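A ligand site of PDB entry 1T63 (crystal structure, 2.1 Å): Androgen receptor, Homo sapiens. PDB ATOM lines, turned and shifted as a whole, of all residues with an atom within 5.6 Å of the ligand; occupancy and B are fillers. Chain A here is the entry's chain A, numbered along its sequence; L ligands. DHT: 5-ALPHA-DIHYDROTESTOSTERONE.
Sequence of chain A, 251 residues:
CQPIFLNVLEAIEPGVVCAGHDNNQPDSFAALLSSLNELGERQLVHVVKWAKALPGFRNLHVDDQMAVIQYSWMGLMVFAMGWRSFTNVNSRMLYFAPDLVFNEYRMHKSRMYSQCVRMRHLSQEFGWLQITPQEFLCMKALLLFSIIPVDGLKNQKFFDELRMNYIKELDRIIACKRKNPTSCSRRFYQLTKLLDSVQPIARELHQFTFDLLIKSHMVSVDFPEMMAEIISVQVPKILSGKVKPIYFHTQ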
ATOM      1  N   LEU A  33      -0.751 -15.586   2.981  1.00  0.00           N
ATOM      2  CA  LEU A  33       0.473 -15.349   3.727  1.00  0.00           C
ATOM      3  C   LEU A  33       1.617 -14.786   2.887  1.00  0.00           C
ATOM      4  O   LEU A  33       2.393 -13.952   3.370  1.00  0.00           O
ATOM      5  CB  LEU A  33       0.912 -16.628   4.458  1.00  0.00           C
ATOM      6  CG  LEU A  33       0.329 -16.732   5.875  1.00  0.00           C
ATOM      7  CD1 LEU A  33       0.782 -15.514   6.695  1.00  0.00           C
ATOM      8  CD2 LEU A  33      -1.191 -16.791   5.821  1.00  0.00           C
ATOM      9  N   LEU A  36       1.007 -11.142   2.707  1.00  0.00           N
ATOM     10  CA  LEU A  36       1.314 -10.448   3.971  1.00  0.00           C
ATOM     11  C   LEU A  36       2.822 -10.210   4.124  1.00  0.00           C
ATOM     12  O   LEU A  36       3.243  -9.154   4.566  1.00  0.00           O
ATOM     13  CB  LEU A  36       0.812 -11.272   5.160  1.00  0.00           C
ATOM     14  CG  LEU A  36      -0.675 -11.170   5.485  1.00  0.00           C
ATOM     15  CD1 LEU A  36      -1.050 -12.240   6.495  1.00  0.00           C
ATOM     16  CD2 LEU A  36      -0.971  -9.777   6.046  1.00  0.00           C
ATOM     17  N   ASN A  37       3.619 -11.225   3.770  1.00  0.00           N
ATOM     18  CA  ASN A  37       5.076 -11.120   3.875  1.00  0.00           C
ATOM     19  C   ASN A  37       5.600 -10.027   2.950  1.00  0.00           C
ATOM     20  O   ASN A  37       6.489  -9.250   3.331  1.00  0.00           O
ATOM     21  CB  ASN A  37       5.761 -12.447   3.507  1.00  0.00           C
ATOM     22  CG  ASN A  37       5.488 -13.561   4.524  1.00  0.00           C
ATOM     23  OD1 ASN A  37       5.387 -13.323   5.723  1.00  0.00           O
ATOM     24  ND2 ASN A  37       5.400 -14.783   4.022  1.00  0.00           N
ATOM     25  N   LEU A  39       3.843  -7.479   1.897  1.00  0.00           N
ATOM     26  CA  LEU A  39       3.377  -6.215   2.476  1.00  0.00           C
ATOM     27  C   LEU A  39       4.351  -5.803   3.582  1.00  0.00           C
ATOM     28  O   LEU A  39       4.645  -4.623   3.764  1.00  0.00           O
ATOM     29  CB  LEU A  39       1.961  -6.369   3.077  1.00  0.00           C
ATOM     30  CG  LEU A  39       1.397  -5.115   3.799  1.00  0.00           C
ATOM     31  CD1 LEU A  39       1.261  -3.979   2.779  1.00  0.00           C
ATOM     32  CD2 LEU A  39       0.030  -5.390   4.443  1.00  0.00           C
ATOM     33  N   GLY A  40       4.844  -6.785   4.328  1.00  0.00           N
ATOM     34  CA  GLY A  40       5.771  -6.493   5.411  1.00  0.00           C
ATOM     35  C   GLY A  40       7.060  -5.860   4.892  1.00  0.00           C
ATOM     36  O   GLY A  40       7.558  -4.886   5.465  1.00  0.00           O
ATOM     37  N   GLN A  43       6.267  -2.215   3.787  1.00  0.00           N
ATOM     38  CA  GLN A  43       6.084  -1.281   4.893  1.00  0.00           C
ATOM     39  C   GLN A  43       7.377  -1.111   5.673  1.00  0.00           C
ATOM     40  O   GLN A  43       7.572  -0.088   6.317  1.00  0.00           O
ATOM     41  CB  GLN A  43       4.988  -1.768   5.846  1.00  0.00           C
ATOM     42  CG  GLN A  43       3.574  -1.690   5.291  1.00  0.00           C
ATOM     43  CD  GLN A  43       2.522  -1.998   6.335  1.00  0.00           C
ATOM     44  OE1 GLN A  43       1.346  -2.184   6.017  1.00  0.00           O
ATOM     45  NE2 GLN A  43       2.924  -2.039   7.596  1.00  0.00           N
ATOM     46  N   TRP A  73       9.436  -3.582  14.651  1.00  0.00           N
ATOM     47  CA  TRP A  73       8.600  -3.456  13.446  1.00  0.00           C
ATOM     48  C   TRP A  73       7.230  -4.137  13.547  1.00  0.00           C
ATOM     49  O   TRP A  73       6.226  -3.574  13.115  1.00  0.00           O
ATOM     50  CB  TRP A  73       9.326  -3.986  12.184  1.00  0.00           C
ATOM     51  CG  TRP A  73       9.718  -5.435  12.225  1.00  0.00           C
ATOM     52  CD1 TRP A  73      10.884  -5.957  12.731  1.00  0.00           C
ATOM     53  CD2 TRP A  73       8.955  -6.549  11.749  1.00  0.00           C
ATOM     54  NE1 TRP A  73      10.895  -7.321  12.584  1.00  0.00           N
ATOM     55  CE2 TRP A  73       9.725  -7.719  11.999  1.00  0.00           C
ATOM     56  CE3 TRP A  73       7.703  -6.682  11.138  1.00  0.00           C
ATOM     57  CZ2 TRP A  73       9.274  -9.007  11.640  1.00  0.00           C
ATOM     58  CZ3 TRP A  73       7.254  -7.963  10.792  1.00  0.00           C
ATOM     59  CH2 TRP A  73       8.039  -9.109  11.042  1.00  0.00           C
ATOM     60  N   MET A  74       7.187  -5.330  14.130  1.00  0.00           N
ATOM     61  CA  MET A  74       5.909  -6.042  14.267  1.00  0.00           C
ATOM     62  C   MET A  74       4.882  -5.204  15.025  1.00  0.00           C
ATOM     63  O   MET A  74       3.781  -4.952  14.535  1.00  0.00           O
ATOM     64  CB  MET A  74       6.124  -7.376  14.991  1.00  0.00           C
ATOM     65  CG  MET A  74       4.878  -8.255  15.067  1.00  0.00           C
ATOM     66  SD  MET A  74       4.347  -8.905  13.473  1.00  0.00           S
ATOM     67  CE  MET A  74       5.458 -10.285  13.303  1.00  0.00           C
ATOM     68  N   MET A  77       3.782  -1.983  13.135  1.00  0.00           N
ATOM     69  CA  MET A  77       2.880  -2.298  12.028  1.00  0.00           C
ATOM     70  C   MET A  77       1.500  -2.767  12.463  1.00  0.00           C
ATOM     71  O   MET A  77       0.509  -2.461  11.804  1.00  0.00           O
ATOM     72  CB  MET A  77       3.516  -3.351  11.119  1.00  0.00           C
ATOM     73  CG  MET A  77       4.723  -2.829  10.365  1.00  0.00           C
ATOM     74  SD  MET A  77       5.476  -4.072   9.255  1.00  0.00           S
ATOM     75  CE  MET A  77       6.986  -3.144   8.766  1.00  0.00           C
ATOM     76  N   VAL A  78       1.431  -3.494  13.577  1.00  0.00           N
ATOM     77  CA  VAL A  78       0.153  -3.959  14.066  1.00  0.00           C
ATOM     78  C   VAL A  78      -0.669  -2.794  14.618  1.00  0.00           C
ATOM     79  O   VAL A  78      -1.879  -2.740  14.435  1.00  0.00           O
ATOM     80  CB  VAL A  78       0.337  -5.036  15.168  1.00  0.00           C
ATOM     81  CG1 VAL A  78      -1.002  -5.369  15.807  1.00  0.00           C
ATOM     82  CG2 VAL A  78       0.953  -6.291  14.544  1.00  0.00           C
ATOM     83  N   MET A  81      -1.907  -0.743  11.634  1.00  0.00           N
ATOM     84  CA  MET A  81      -2.969  -1.509  10.982  1.00  0.00           C
ATOM     85  C   MET A  81      -4.264  -1.418  11.788  1.00  0.00           C
ATOM     86  O   MET A  81      -5.357  -1.343  11.223  1.00  0.00           O
ATOM     87  CB  MET A  81      -2.527  -2.974  10.796  1.00  0.00           C
ATOM     88  CG  MET A  81      -3.495  -3.850   9.969  1.00  0.00           C
ATOM     89  SD  MET A  81      -4.945  -4.494  10.870  1.00  0.00           S
ATOM     90  CE  MET A  81      -4.139  -5.762  11.927  1.00  0.00           C
ATOM     91  N   ARG A  84      -5.848   1.918  11.031  1.00  0.00           N
ATOM     92  CA  ARG A  84      -6.428   1.935   9.689  1.00  0.00           C
ATOM     93  C   ARG A  84      -7.772   1.232   9.684  1.00  0.00           C
ATOM     94  O   ARG A  84      -8.718   1.684   9.035  1.00  0.00           O
ATOM     95  CB  ARG A  84      -5.535   1.200   8.676  1.00  0.00           C
ATOM     96  CG  ARG A  84      -4.283   1.927   8.234  1.00  0.00           C
ATOM     97  CD  ARG A  84      -3.732   1.263   6.960  1.00  0.00           C
ATOM     98  NE  ARG A  84      -3.206  -0.088   7.163  1.00  0.00           N
ATOM     99  CZ  ARG A  84      -2.050  -0.360   7.776  1.00  0.00           C
ATOM    100  NH1 ARG A  84      -1.297   0.621   8.238  1.00  0.00           N
ATOM    101  NH2 ARG A  84      -1.626  -1.615   7.877  1.00  0.00           N
ATOM    102  N   TYR A  95      -7.897  -4.075   8.070  1.00  0.00           N
ATOM    103  CA  TYR A  95      -7.428  -3.347   6.899  1.00  0.00           C
ATOM    104  C   TYR A  95      -5.904  -3.344   6.804  1.00  0.00           C
ATOM    105  O   TYR A  95      -5.267  -2.348   7.122  1.00  0.00           O
ATOM    106  CB  TYR A  95      -7.969  -1.901   6.958  1.00  0.00           C
ATOM    107  CG  TYR A  95      -8.041  -1.166   5.626  1.00  0.00           C
ATOM    108  CD1 TYR A  95      -6.886  -0.707   4.997  1.00  0.00           C
ATOM    109  CD2 TYR A  95      -9.270  -0.926   5.009  1.00  0.00           C
ATOM    110  CE1 TYR A  95      -6.942  -0.026   3.774  1.00  0.00           C
ATOM    111  CE2 TYR A  95      -9.342  -0.251   3.776  1.00  0.00           C
ATOM    112  CZ  TYR A  95      -8.175   0.192   3.178  1.00  0.00           C
ATOM    113  OH  TYR A  95      -8.213   0.862   1.975  1.00  0.00           O
ATOM    114  N   PHE A  96      -5.327  -4.472   6.377  1.00  0.00           N
ATOM    115  CA  PHE A  96      -3.875  -4.581   6.233  1.00  0.00           C
ATOM    116  C   PHE A  96      -3.381  -3.623   5.127  1.00  0.00           C
ATOM    117  O   PHE A  96      -2.396  -2.915   5.302  1.00  0.00           O
ATOM    118  CB  PHE A  96      -3.472  -6.037   5.901  1.00  0.00           C
ATOM    119  CG  PHE A  96      -3.621  -6.997   7.059  1.00  0.00           C
ATOM    120  CD1 PHE A  96      -2.766  -6.934   8.148  1.00  0.00           C
ATOM    121  CD2 PHE A  96      -4.618  -7.974   7.042  1.00  0.00           C
ATOM    122  CE1 PHE A  96      -2.886  -7.811   9.223  1.00  0.00           C
ATOM    123  CE2 PHE A  96      -4.767  -8.867   8.113  1.00  0.00           C
ATOM    124  CZ  PHE A  96      -3.897  -8.788   9.208  1.00  0.00           C
ATOM    125  N   MET A 112      -4.544 -18.108  11.278  1.00  0.00           N
ATOM    126  CA  MET A 112      -4.154 -17.297  12.432  1.00  0.00           C
ATOM    127  C   MET A 112      -5.357 -16.495  12.895  1.00  0.00           C
ATOM    128  O   MET A 112      -5.269 -15.300  13.136  1.00  0.00           O
ATOM    129  CB  MET A 112      -2.965 -16.386  12.086  1.00  0.00           C
ATOM    130  CG  MET A 112      -3.007 -15.743  10.727  1.00  0.00           C
ATOM    131  SD  MET A 112      -1.482 -14.795  10.379  1.00  0.00           S
ATOM    132  CE  MET A 112      -1.989 -13.132  10.859  1.00  0.00           C
ATOM    133  N   MET A 119      -6.105  -8.659  17.246  1.00  0.00           N
ATOM    134  CA  MET A 119      -5.825  -7.439  16.487  1.00  0.00           C
ATOM    135  C   MET A 119      -7.103  -6.642  16.256  1.00  0.00           C
ATOM    136  O   MET A 119      -7.096  -5.419  16.348  1.00  0.00           O
ATOM    137  CB  MET A 119      -5.153  -7.786  15.150  1.00  0.00           C
ATOM    138  CG  MET A 119      -3.745  -8.338  15.289  1.00  0.00           C
ATOM    139  SD  MET A 119      -2.800  -8.456  13.724  1.00  0.00           S
ATOM    140  CE  MET A 119      -3.295 -10.101  13.153  1.00  0.00           C
ATOM    141  N   LEU A 205       2.478 -13.083  17.117  1.00  0.00           N
ATOM    142  CA  LEU A 205       2.753 -12.983  15.696  1.00  0.00           C
ATOM    143  C   LEU A 205       4.207 -13.345  15.397  1.00  0.00           C
ATOM    144  O   LEU A 205       4.512 -13.875  14.326  1.00  0.00           O
ATOM    145  CB  LEU A 205       2.451 -11.569  15.194  1.00  0.00           C
ATOM    146  CG  LEU A 205       0.952 -11.219  15.075  1.00  0.00           C
ATOM    147  CD1 LEU A 205       0.785  -9.764  14.651  1.00  0.00           C
ATOM    148  CD2 LEU A 205       0.290 -12.159  14.061  1.00  0.00           C
ATOM    149  N   PHE A 208       4.413 -17.132  15.396  1.00  0.00           N
ATOM    150  CA  PHE A 208       3.766 -17.639  14.190  1.00  0.00           C
ATOM    151  C   PHE A 208       4.628 -17.467  12.943  1.00  0.00           C
ATOM    152  O   PHE A 208       4.791 -18.396  12.165  1.00  0.00           O
ATOM    153  CB  PHE A 208       2.406 -16.958  13.988  1.00  0.00           C
ATOM    154  CG  PHE A 208       1.619 -17.488  12.802  1.00  0.00           C
ATOM    155  CD1 PHE A 208       1.887 -17.058  11.509  1.00  0.00           C
ATOM    156  CD2 PHE A 208       0.592 -18.411  12.997  1.00  0.00           C
ATOM    157  CE1 PHE A 208       1.157 -17.526  10.410  1.00  0.00           C
ATOM    158  CE2 PHE A 208      -0.165 -18.896  11.911  1.00  0.00           C
ATOM    159  CZ  PHE A 208       0.124 -18.445  10.612  1.00  0.00           C
ATOM    160  N   THR A 209       5.191 -16.283  12.753  1.00  0.00           N
ATOM    161  CA  THR A 209       6.012 -16.071  11.565  1.00  0.00           C
ATOM    162  C   THR A 209       7.291 -16.906  11.620  1.00  0.00           C
ATOM    163  O   THR A 209       7.741 -17.441  10.602  1.00  0.00           O
ATOM    164  CB  THR A 209       6.345 -14.566  11.350  1.00  0.00           C
ATOM    165  OG1 THR A 209       6.880 -14.378  10.033  1.00  0.00           O
ATOM    166  CG2 THR A 209       7.334 -14.063  12.371  1.00  0.00           C
ATOM    167  N   LEU A 212       6.457 -20.432  10.609  1.00  0.00           N
ATOM    168  CA  LEU A 212       6.163 -20.486   9.177  1.00  0.00           C
ATOM    169  C   LEU A 212       7.457 -20.402   8.357  1.00  0.00           C
ATOM    170  O   LEU A 212       7.565 -21.027   7.306  1.00  0.00           O
ATOM    171  CB  LEU A 212       5.212 -19.337   8.789  1.00  0.00           C
ATOM    172  CG  LEU A 212       4.783 -19.234   7.310  1.00  0.00           C
ATOM    173  CD1 LEU A 212       4.223 -20.560   6.811  1.00  0.00           C
ATOM    174  CD2 LEU A 212       3.741 -18.126   7.155  1.00  0.00           C
ATOM    175  N   PHE A 223       9.177 -15.688   1.523  1.00  0.00           N
ATOM    176  CA  PHE A 223       9.603 -14.655   2.449  1.00  0.00           C
ATOM    177  C   PHE A 223      10.622 -13.740   1.754  1.00  0.00           C
ATOM    178  O   PHE A 223      11.621 -14.212   1.215  1.00  0.00           O
ATOM    179  CB  PHE A 223      10.245 -15.259   3.705  1.00  0.00           C
ATOM    180  CG  PHE A 223       9.247 -15.830   4.697  1.00  0.00           C
ATOM    181  CD1 PHE A 223       8.574 -17.020   4.427  1.00  0.00           C
ATOM    182  CD2 PHE A 223       9.002 -15.184   5.914  1.00  0.00           C
ATOM    183  CE1 PHE A 223       7.658 -17.556   5.345  1.00  0.00           C
ATOM    184  CE2 PHE A 223       8.093 -15.707   6.832  1.00  0.00           C
ATOM    185  CZ  PHE A 223       7.417 -16.895   6.545  1.00  0.00           C
ATOM    186  N   ILE A 231      13.700 -12.359  10.694  1.00  0.00           N
ATOM    187  CA  ILE A 231      12.978 -13.411  11.408  1.00  0.00           C
ATOM    188  C   ILE A 231      13.873 -14.578  11.856  1.00  0.00           C
ATOM    189  O   ILE A 231      13.637 -15.179  12.911  1.00  0.00           O
ATOM    190  CB  ILE A 231      11.809 -13.925  10.520  1.00  0.00           C
ATOM    191  CG1 ILE A 231      10.889 -12.755  10.188  1.00  0.00           C
ATOM    192  CG2 ILE A 231      11.036 -15.037  11.235  1.00  0.00           C
ATOM    193  CD1 ILE A 231       9.829 -13.026   9.124  1.00  0.00           C
HETATM  194  C1  DHT L   1       2.096  -6.680   7.557  1.00  0.00           C
HETATM  195  C2  DHT L   1       1.863  -5.175   7.744  1.00  0.00           C
HETATM  196  C3  DHT L   1       0.589  -5.033   8.641  1.00  0.00           C
HETATM  197  O3  DHT L   1      -0.307  -4.280   8.250  1.00  0.00           O
HETATM  198  C4  DHT L   1       0.506  -5.822   9.897  1.00  0.00           C
HETATM  199  C5  DHT L   1       0.728  -7.343   9.639  1.00  0.00           C
HETATM  200  C6  DHT L   1       0.665  -8.210  10.934  1.00  0.00           C
HETATM  201  C7  DHT L   1       0.880  -9.700  10.587  1.00  0.00           C
HETATM  202  C8  DHT L   1       2.221  -9.968   9.847  1.00  0.00           C
HETATM  203  C9  DHT L   1       2.290  -9.080   8.547  1.00  0.00           C
HETATM  204  C10 DHT L   1       2.127  -7.537   8.857  1.00  0.00           C
HETATM  205  C11 DHT L   1       3.622  -9.400   7.796  1.00  0.00           C
HETATM  206  C12 DHT L   1       3.907 -10.867   7.482  1.00  0.00           C
HETATM  207  C13 DHT L   1       3.727 -11.786   8.719  1.00  0.00           C
HETATM  208  C14 DHT L   1       2.371 -11.435   9.448  1.00  0.00           C
HETATM  209  C15 DHT L   1       2.343 -12.484  10.569  1.00  0.00           C
HETATM  210  C16 DHT L   1       2.744 -13.762   9.806  1.00  0.00           C
HETATM  211  C17 DHT L   1       3.441 -13.267   8.506  1.00  0.00           C
HETATM  212  O17 DHT L   1       4.618 -14.043   8.285  1.00  0.00           O
HETATM  213  C18 DHT L   1       4.977 -11.594   9.673  1.00  0.00           C
HETATM  214  C19 DHT L   1       3.330  -7.060   9.776  1.00  0.00           C
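NE2 of Gln 43 sits close to SD of Met 77.
The side-chain amide nitrogen of Asn 37 is in hydrogen-bond range of the backbone carbonyl oxygen of Leu 33, 3.2 Å away.
NE of Arg 84 lies within hydrogen-bond range of O of Tyr 95, 3.1 Å away.
The guanidinium group of Arg 84 lies within hydrogen-bond range of the backbone carbonyl oxygen of Phe 96 (3.0 Å).
The side-chain amide oxygen (OE1) of Gln 43 lies close to an oxygen (O3) of the ligand, at 3.5 Å.
O17 of the ligand lies within hydrogen-bond range of OG1 of Thr 209.
The guanidinium group of Arg 84 lies within hydrogen-bond range of an oxygen (O3) of the ligand, 3.0 Å away.
The side-chain amide oxygen (OD1) of Asn 37 lies within hydrogen-bond range of an oxygen (O17) of the ligand (2.8 Å).
Merely in contact with the ligand: Leu 36, Phe 96, Met 81, Met 77, Leu 39, Phe 208, Met 74 and Leu 33.
Hydrophobic or aromatic side chains that line the ligand: Leu 33, Leu 36, Leu 39, Met 74, Met 77, Met 81, Phe 96 and Phe 208.
Within 4 Å of the ligand: Leu 33, Leu 36, Asn 37, Leu 39, Gln 43, Met 74, Met 77, Met 81, Arg 84, Phe 96, Phe 208 and Thr 209.
Along chain A the residues within 4 Å of the ligand span positions 33 to 209.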
